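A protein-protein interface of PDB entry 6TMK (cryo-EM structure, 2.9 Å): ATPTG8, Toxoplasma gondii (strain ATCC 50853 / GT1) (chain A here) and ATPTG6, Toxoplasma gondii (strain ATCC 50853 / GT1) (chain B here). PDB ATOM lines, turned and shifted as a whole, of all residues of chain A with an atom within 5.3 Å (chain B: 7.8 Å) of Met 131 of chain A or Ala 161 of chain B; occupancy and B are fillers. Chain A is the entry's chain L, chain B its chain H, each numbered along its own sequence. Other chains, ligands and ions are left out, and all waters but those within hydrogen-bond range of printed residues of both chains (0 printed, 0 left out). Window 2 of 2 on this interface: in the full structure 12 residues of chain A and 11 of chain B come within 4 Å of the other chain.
Among the printed residues, pairs that only touch across the chains: Met 131 of chain A with Lys 158 of chain B (3.9 Å), Met 131 of chain A with Ala 161 of chain B (3.7 Å) and Val 134 of chain A with Asp 162 of chain B (3.6 Å).
Of the 11 printed residues of chain A, 4 touch a printed residue of chain B.
Printed residues of chain A that touch a printed residue of chain B: Arg 130, Met 131, Val 134 and Arg 138.
Hydrophobic or aromatic side chains of chain A that line the printed part of chain B: Met 131 and Val 134.
Hydrophobic or aromatic side chains of chain B that line the printed part of chain A: Ala 161.
Among the printed residues, 7 pairs touch across the chains.
Among the printed residues, Asp or Glu carboxylates within 4 Å of a Lys or Arg side-chain nitrogen of the other chain: Arg 130 of chain A with Asp 162 of chain B (3.1 Å) and Arg 138 of chain A with Asp 163 of chain B (3.6 Å).
Of the printed residues of chain B, Arg 130 of chain A touches Asp 162 (3.1 Å).
Of chain B, only Lys 158 (3.9 Å) and Ala 161 (3.7 Å) come within 4 Å of Met 131 of chain A.
Printed residues of chain B within 4 Å of Val 134 of chain A: Asp 162.
Of the printed residues of chain B, Arg 138 of chain A touches Ala 161 (3.4 Å), Asp 162 (2.4 Å) and Asp 163 (3.6 Å).
Printed residues of chain A within 4 Å of Ala 161 of chain B: Met 131 (3.7 Å) and Arg 138 (3.4 Å).
Of the printed residues of chain A, Asp 162 of chain B touches Arg 130 (3.1 Å), Val 134 (3.6 Å) and Arg 138 (2.4 Å).
The nearest residue of chain B that does not touch Met 131 of chain A is Asp 162 of chain B (5.2 Å).
The guanidinium group (NH2) of Arg 138 of chain A lies close to the backbone carbonyl oxygen (O) of Asp 162 of chain B (2.4 Å).
OD1 of Asp 162 of chain B is in salt-bridge range of NE of Arg 130 of chain A, at 3.1 Å.
The side-chain carboxylate (OD1) of Asp 163 of chain B lies within salt-bridge range of the guanidinium group (NH1) of Arg 138 of chain A.
The backbone carbonyl oxygen (O) of Ala 161 of chain B lies within hydrogen-bond range of the guanidinium group (NH2) of Arg 138 of chain A (3.4 Å).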
ATOM      1  N   ASN A 127      -1.966 -16.563  -1.020  1.00  0.00           N
ATOM      2  CA  ASN A 127      -0.593 -16.962  -1.267  1.00  0.00           C
ATOM      3  C   ASN A 127      -0.550 -18.411  -1.752  1.00  0.00           C
ATOM      4  O   ASN A 127      -1.274 -19.260  -1.227  1.00  0.00           O
ATOM      5  CB  ASN A 127       0.233 -16.802   0.002  1.00  0.00           C
ATOM      6  CG  ASN A 127       1.716 -16.821  -0.257  1.00  0.00           C
ATOM      7  OD1 ASN A 127       2.243 -17.731  -0.891  1.00  0.00           O
ATOM      8  ND2 ASN A 127       2.403 -15.810   0.238  1.00  0.00           N
ATOM      9  N   PRO A 128       0.278 -18.727  -2.750  1.00  0.00           N
ATOM     10  CA  PRO A 128       0.343 -20.123  -3.204  1.00  0.00           C
ATOM     11  C   PRO A 128       1.069 -21.054  -2.247  1.00  0.00           C
ATOM     12  O   PRO A 128       0.721 -22.239  -2.186  1.00  0.00           O
ATOM     13  CB  PRO A 128       1.080 -20.020  -4.547  1.00  0.00           C
ATOM     14  CG  PRO A 128       1.004 -18.600  -4.930  1.00  0.00           C
ATOM     15  CD  PRO A 128       0.986 -17.831  -3.673  1.00  0.00           C
ATOM     16  N   CYS A 129       2.070 -20.573  -1.513  1.00  0.00           N
ATOM     17  CA  CYS A 129       2.862 -21.451  -0.660  1.00  0.00           C
ATOM     18  C   CYS A 129       2.173 -21.785   0.658  1.00  0.00           C
ATOM     19  O   CYS A 129       2.687 -22.620   1.418  1.00  0.00           O
ATOM     20  CB  CYS A 129       4.221 -20.809  -0.379  1.00  0.00           C
ATOM     21  SG  CYS A 129       5.086 -20.171  -1.833  1.00  0.00           S
ATOM     22  N   ARG A 130       1.018 -21.181   0.930  1.00  0.00           N
ATOM     23  CA  ARG A 130       0.342 -21.394   2.203  1.00  0.00           C
ATOM     24  C   ARG A 130      -0.072 -22.844   2.390  1.00  0.00           C
ATOM     25  O   ARG A 130       0.154 -23.431   3.453  1.00  0.00           O
ATOM     26  CB  ARG A 130      -0.871 -20.481   2.303  1.00  0.00           C
ATOM     27  CG  ARG A 130      -1.441 -20.394   3.693  1.00  0.00           C
ATOM     28  CD  ARG A 130      -2.859 -19.939   3.660  1.00  0.00           C
ATOM     29  NE  ARG A 130      -3.526 -20.117   4.941  1.00  0.00           N
ATOM     30  CZ  ARG A 130      -3.416 -19.289   5.968  1.00  0.00           C
ATOM     31  NH1 ARG A 130      -2.657 -18.215   5.887  1.00  0.00           N
ATOM     32  NH2 ARG A 130      -4.065 -19.540   7.086  1.00  0.00           N
ATOM     33  N   MET A 131      -0.713 -23.431   1.385  1.00  0.00           N
ATOM     34  CA  MET A 131      -1.174 -24.808   1.528  1.00  0.00           C
ATOM     35  C   MET A 131      -0.023 -25.782   1.705  1.00  0.00           C
ATOM     36  O   MET A 131      -0.092 -26.629   2.612  1.00  0.00           O
ATOM     37  CB  MET A 131      -2.044 -25.186   0.327  1.00  0.00           C
ATOM     38  CG  MET A 131      -3.527 -25.009   0.563  1.00  0.00           C
ATOM     39  SD  MET A 131      -4.551 -25.685  -0.751  1.00  0.00           S
ATOM     40  CE  MET A 131      -4.673 -24.284  -1.850  1.00  0.00           C
ATOM     41  N   PRO A 132       1.036 -25.740   0.896  1.00  0.00           N
ATOM     42  CA  PRO A 132       2.183 -26.615   1.163  1.00  0.00           C
ATOM     43  C   PRO A 132       2.806 -26.406   2.529  1.00  0.00           C
ATOM     44  O   PRO A 132       3.149 -27.387   3.202  1.00  0.00           O
ATOM     45  CB  PRO A 132       3.153 -26.245   0.039  1.00  0.00           C
ATOM     46  CG  PRO A 132       2.313 -25.774  -1.040  1.00  0.00           C
ATOM     47  CD  PRO A 132       1.131 -25.111  -0.427  1.00  0.00           C
ATOM     48  N   GLY A 133       2.967 -25.156   2.965  1.00  0.00           N
ATOM     49  CA  GLY A 133       3.549 -24.926   4.275  1.00  0.00           C
ATOM     50  C   GLY A 133       2.705 -25.499   5.393  1.00  0.00           C
ATOM     51  O   GLY A 133       3.213 -26.156   6.309  1.00  0.00           O
ATOM     52  N   VAL A 134       1.397 -25.259   5.331  1.00  0.00           N
ATOM     53  CA  VAL A 134       0.502 -25.764   6.360  1.00  0.00           C
ATOM     54  C   VAL A 134       0.484 -27.283   6.346  1.00  0.00           C
ATOM     55  O   VAL A 134       0.422 -27.925   7.399  1.00  0.00           O
ATOM     56  CB  VAL A 134      -0.906 -25.177   6.172  1.00  0.00           C
ATOM     57  CG1 VAL A 134      -1.873 -25.838   7.106  1.00  0.00           C
ATOM     58  CG2 VAL A 134      -0.889 -23.691   6.397  1.00  0.00           C
ATOM     59  N   ALA A 135       0.554 -27.884   5.159  1.00  0.00           N
ATOM     60  CA  ALA A 135       0.583 -29.336   5.068  1.00  0.00           C
ATOM     61  C   ALA A 135       1.846 -29.902   5.700  1.00  0.00           C
ATOM     62  O   ALA A 135       1.795 -30.902   6.426  1.00  0.00           O
ATOM     63  CB  ALA A 135       0.467 -29.762   3.610  1.00  0.00           C
ATOM     64  N   TYR A 136       2.992 -29.275   5.437  1.00  0.00           N
ATOM     65  CA  TYR A 136       4.243 -29.756   6.008  1.00  0.00           C
ATOM     66  C   TYR A 136       4.232 -29.644   7.526  1.00  0.00           C
ATOM     67  O   TYR A 136       4.661 -30.565   8.233  1.00  0.00           O
ATOM     68  CB  TYR A 136       5.419 -28.987   5.418  1.00  0.00           C
ATOM     69  CG  TYR A 136       6.744 -29.368   6.022  1.00  0.00           C
ATOM     70  CD1 TYR A 136       7.251 -30.643   5.867  1.00  0.00           C
ATOM     71  CD2 TYR A 136       7.492 -28.455   6.739  1.00  0.00           C
ATOM     72  CE1 TYR A 136       8.455 -30.999   6.411  1.00  0.00           C
ATOM     73  CE2 TYR A 136       8.699 -28.805   7.288  1.00  0.00           C
ATOM     74  CZ  TYR A 136       9.177 -30.077   7.121  1.00  0.00           C
ATOM     75  OH  TYR A 136      10.385 -30.433   7.668  1.00  0.00           O
ATOM     76  N   ARG A 138       1.572 -29.610   9.414  1.00  0.00           N
ATOM     77  CA  ARG A 138       0.621 -30.602   9.894  1.00  0.00           C
ATOM     78  C   ARG A 138       1.255 -31.985   9.941  1.00  0.00           C
ATOM     79  O   ARG A 138       0.991 -32.767  10.858  1.00  0.00           O
ATOM     80  CB  ARG A 138      -0.596 -30.609   8.982  1.00  0.00           C
ATOM     81  CG  ARG A 138      -1.880 -31.057   9.614  1.00  0.00           C
ATOM     82  CD  ARG A 138      -2.952 -31.174   8.553  1.00  0.00           C
ATOM     83  NE  ARG A 138      -3.281 -29.875   7.979  1.00  0.00           N
ATOM     84  CZ  ARG A 138      -4.104 -28.995   8.534  1.00  0.00           C
ATOM     85  NH1 ARG A 138      -4.696 -29.265   9.688  1.00  0.00           N
ATOM     86  NH2 ARG A 138      -4.334 -27.840   7.933  1.00  0.00           N
ATOM     87  N   ASP B 154     -13.981 -22.263  -4.812  1.00  0.00           N
ATOM     88  CA  ASP B 154     -12.527 -22.316  -4.723  1.00  0.00           C
ATOM     89  C   ASP B 154     -12.045 -21.847  -3.354  1.00  0.00           C
ATOM     90  O   ASP B 154     -11.176 -22.475  -2.733  1.00  0.00           O
ATOM     91  CB  ASP B 154     -11.913 -21.467  -5.833  1.00  0.00           C
ATOM     92  CG  ASP B 154     -11.836 -22.203  -7.159  1.00  0.00           C
ATOM     93  OD1 ASP B 154     -12.207 -23.395  -7.209  1.00  0.00           O
ATOM     94  OD2 ASP B 154     -11.403 -21.591  -8.155  1.00  0.00           O
ATOM     95  N   PHE B 155     -12.604 -20.737  -2.869  1.00  0.00           N
ATOM     96  CA  PHE B 155     -12.231 -20.232  -1.553  1.00  0.00           C
ATOM     97  C   PHE B 155     -12.564 -21.238  -0.461  1.00  0.00           C
ATOM     98  O   PHE B 155     -11.784 -21.434   0.479  1.00  0.00           O
ATOM     99  CB  PHE B 155     -12.934 -18.897  -1.311  1.00  0.00           C
ATOM    100  CG  PHE B 155     -12.670 -18.302   0.028  1.00  0.00           C
ATOM    101  CD1 PHE B 155     -11.488 -17.647   0.284  1.00  0.00           C
ATOM    102  CD2 PHE B 155     -13.608 -18.387   1.030  1.00  0.00           C
ATOM    103  CE1 PHE B 155     -11.247 -17.100   1.510  1.00  0.00           C
ATOM    104  CE2 PHE B 155     -13.367 -17.842   2.256  1.00  0.00           C
ATOM    105  CZ  PHE B 155     -12.190 -17.196   2.500  1.00  0.00           C
ATOM    106  N   ALA B 156     -13.724 -21.887  -0.567  1.00  0.00           N
ATOM    107  CA  ALA B 156     -14.115 -22.888   0.415  1.00  0.00           C
ATOM    108  C   ALA B 156     -13.159 -24.071   0.410  1.00  0.00           C
ATOM    109  O   ALA B 156     -12.797 -24.592   1.470  1.00  0.00           O
ATOM    110  CB  ALA B 156     -15.538 -23.347   0.136  1.00  0.00           C
ATOM    111  N   ALA B 157     -12.750 -24.518  -0.776  1.00  0.00           N
ATOM    112  CA  ALA B 157     -11.778 -25.598  -0.862  1.00  0.00           C
ATOM    113  C   ALA B 157     -10.468 -25.205  -0.194  1.00  0.00           C
ATOM    114  O   ALA B 157      -9.881 -25.987   0.564  1.00  0.00           O
ATOM    115  CB  ALA B 157     -11.553 -25.970  -2.323  1.00  0.00           C
ATOM    116  N   LYS B 158      -9.992 -23.989  -0.468  1.00  0.00           N
ATOM    117  CA  LYS B 158      -8.740 -23.541   0.128  1.00  0.00           C
ATOM    118  C   LYS B 158      -8.846 -23.461   1.644  1.00  0.00           C
ATOM    119  O   LYS B 158      -7.902 -23.811   2.360  1.00  0.00           O
ATOM    120  CB  LYS B 158      -8.336 -22.193  -0.458  1.00  0.00           C
ATOM    121  CG  LYS B 158      -7.968 -22.260  -1.920  1.00  0.00           C
ATOM    122  CD  LYS B 158      -7.672 -20.898  -2.496  1.00  0.00           C
ATOM    123  CE  LYS B 158      -7.432 -20.989  -3.989  1.00  0.00           C
ATOM    124  NZ  LYS B 158      -8.276 -20.052  -4.770  1.00  0.00           N
ATOM    125  N   VAL B 159      -9.995 -23.029   2.158  1.00  0.00           N
ATOM    126  CA  VAL B 159     -10.148 -22.898   3.601  1.00  0.00           C
ATOM    127  C   VAL B 159     -10.213 -24.273   4.255  1.00  0.00           C
ATOM    128  O   VAL B 159      -9.611 -24.511   5.313  1.00  0.00           O
ATOM    129  CB  VAL B 159     -11.399 -22.060   3.915  1.00  0.00           C
ATOM    130  CG1 VAL B 159     -11.785 -22.192   5.358  1.00  0.00           C
ATOM    131  CG2 VAL B 159     -11.163 -20.621   3.576  1.00  0.00           C
ATOM    132  N   HIS B 160     -10.947 -25.196   3.635  1.00  0.00           N
ATOM    133  CA  HIS B 160     -11.012 -26.558   4.139  1.00  0.00           C
ATOM    134  C   HIS B 160      -9.636 -27.203   4.160  1.00  0.00           C
ATOM    135  O   HIS B 160      -9.307 -27.952   5.086  1.00  0.00           O
ATOM    136  CB  HIS B 160     -11.966 -27.373   3.276  1.00  0.00           C
ATOM    137  CG  HIS B 160     -12.352 -28.684   3.876  1.00  0.00           C
ATOM    138  ND1 HIS B 160     -12.883 -28.794   5.141  1.00  0.00           N
ATOM    139  CD2 HIS B 160     -12.276 -29.943   3.388  1.00  0.00           C
ATOM    140  CE1 HIS B 160     -13.125 -30.064   5.404  1.00  0.00           C
ATOM    141  NE2 HIS B 160     -12.766 -30.783   4.357  1.00  0.00           N
ATOM    142  N   ALA B 161      -8.820 -26.933   3.142  1.00  0.00           N
ATOM    143  CA  ALA B 161      -7.451 -27.431   3.145  1.00  0.00           C
ATOM    144  C   ALA B 161      -6.621 -26.768   4.235  1.00  0.00           C
ATOM    145  O   ALA B 161      -5.772 -27.416   4.855  1.00  0.00           O
ATOM    146  CB  ALA B 161      -6.812 -27.202   1.781  1.00  0.00           C
ATOM    147  N   ASP B 162      -6.853 -25.481   4.483  1.00  0.00           N
ATOM    148  CA  ASP B 162      -6.103 -24.786   5.521  1.00  0.00           C
ATOM    149  C   ASP B 162      -6.349 -25.420   6.881  1.00  0.00           C
ATOM    150  O   ASP B 162      -5.401 -25.764   7.596  1.00  0.00           O
ATOM    151  CB  ASP B 162      -6.482 -23.308   5.542  1.00  0.00           C
ATOM    152  CG  ASP B 162      -5.731 -22.529   6.594  1.00  0.00           C
ATOM    153  OD1 ASP B 162      -4.484 -22.534   6.562  1.00  0.00           O
ATOM    154  OD2 ASP B 162      -6.387 -21.909   7.453  1.00  0.00           O
ATOM    155  N   ASP B 163      -7.613 -25.591   7.254  1.00  0.00           N
ATOM    156  CA  ASP B 163      -7.880 -26.385   8.447  1.00  0.00           C
ATOM    157  C   ASP B 163      -9.291 -26.957   8.435  1.00  0.00           C
ATOM    158  O   ASP B 163     -10.269 -26.200   8.431  1.00  0.00           O
ATOM    159  CB  ASP B 163      -7.664 -25.546   9.705  1.00  0.00           C
ATOM    160  CG  ASP B 163      -7.495 -26.396  10.950  1.00  0.00           C
ATOM    161  OD1 ASP B 163      -7.704 -27.624  10.868  1.00  0.00           O
ATOM    162  OD2 ASP B 163      -7.152 -25.836  12.012  1.00  0.00           O
ATOM    163  N   PRO B 164      -9.439 -28.285   8.439  1.00  0.00           N
ATOM    164  CA  PRO B 164     -10.788 -28.855   8.568  1.00  0.00           C
ATOM    165  C   PRO B 164     -11.365 -28.716   9.961  1.00  0.00           C
ATOM    166  O   PRO B 164     -12.565 -28.454  10.104  1.00  0.00           O
ATOM    167  CB  PRO B 164     -10.581 -30.325   8.179  1.00  0.00           C
ATOM    168  CG  PRO B 164      -9.258 -30.368   7.488  1.00  0.00           C
ATOM    169  CD  PRO B 164      -8.445 -29.318   8.128  1.00  0.00           C
ATOM    170  N   LYS B 169     -14.924 -21.831  10.115  1.00  0.00           N
ATOM    171  CA  LYS B 169     -14.739 -22.100   8.695  1.00  0.00           C
ATOM    172  C   LYS B 169     -15.893 -21.555   7.862  1.00  0.00           C
ATOM    173  O   LYS B 169     -15.708 -20.707   6.977  1.00  0.00           O
ATOM    174  CB  LYS B 169     -14.590 -23.606   8.512  1.00  0.00           C
ATOM    175  CG  LYS B 169     -14.554 -24.096   7.110  1.00  0.00           C
ATOM    176  CD  LYS B 169     -13.954 -25.472   7.057  1.00  0.00           C
ATOM    177  CE  LYS B 169     -14.822 -26.460   7.797  1.00  0.00           C
ATOM    178  NZ  LYS B 169     -14.482 -27.864   7.491  1.00  0.00           N
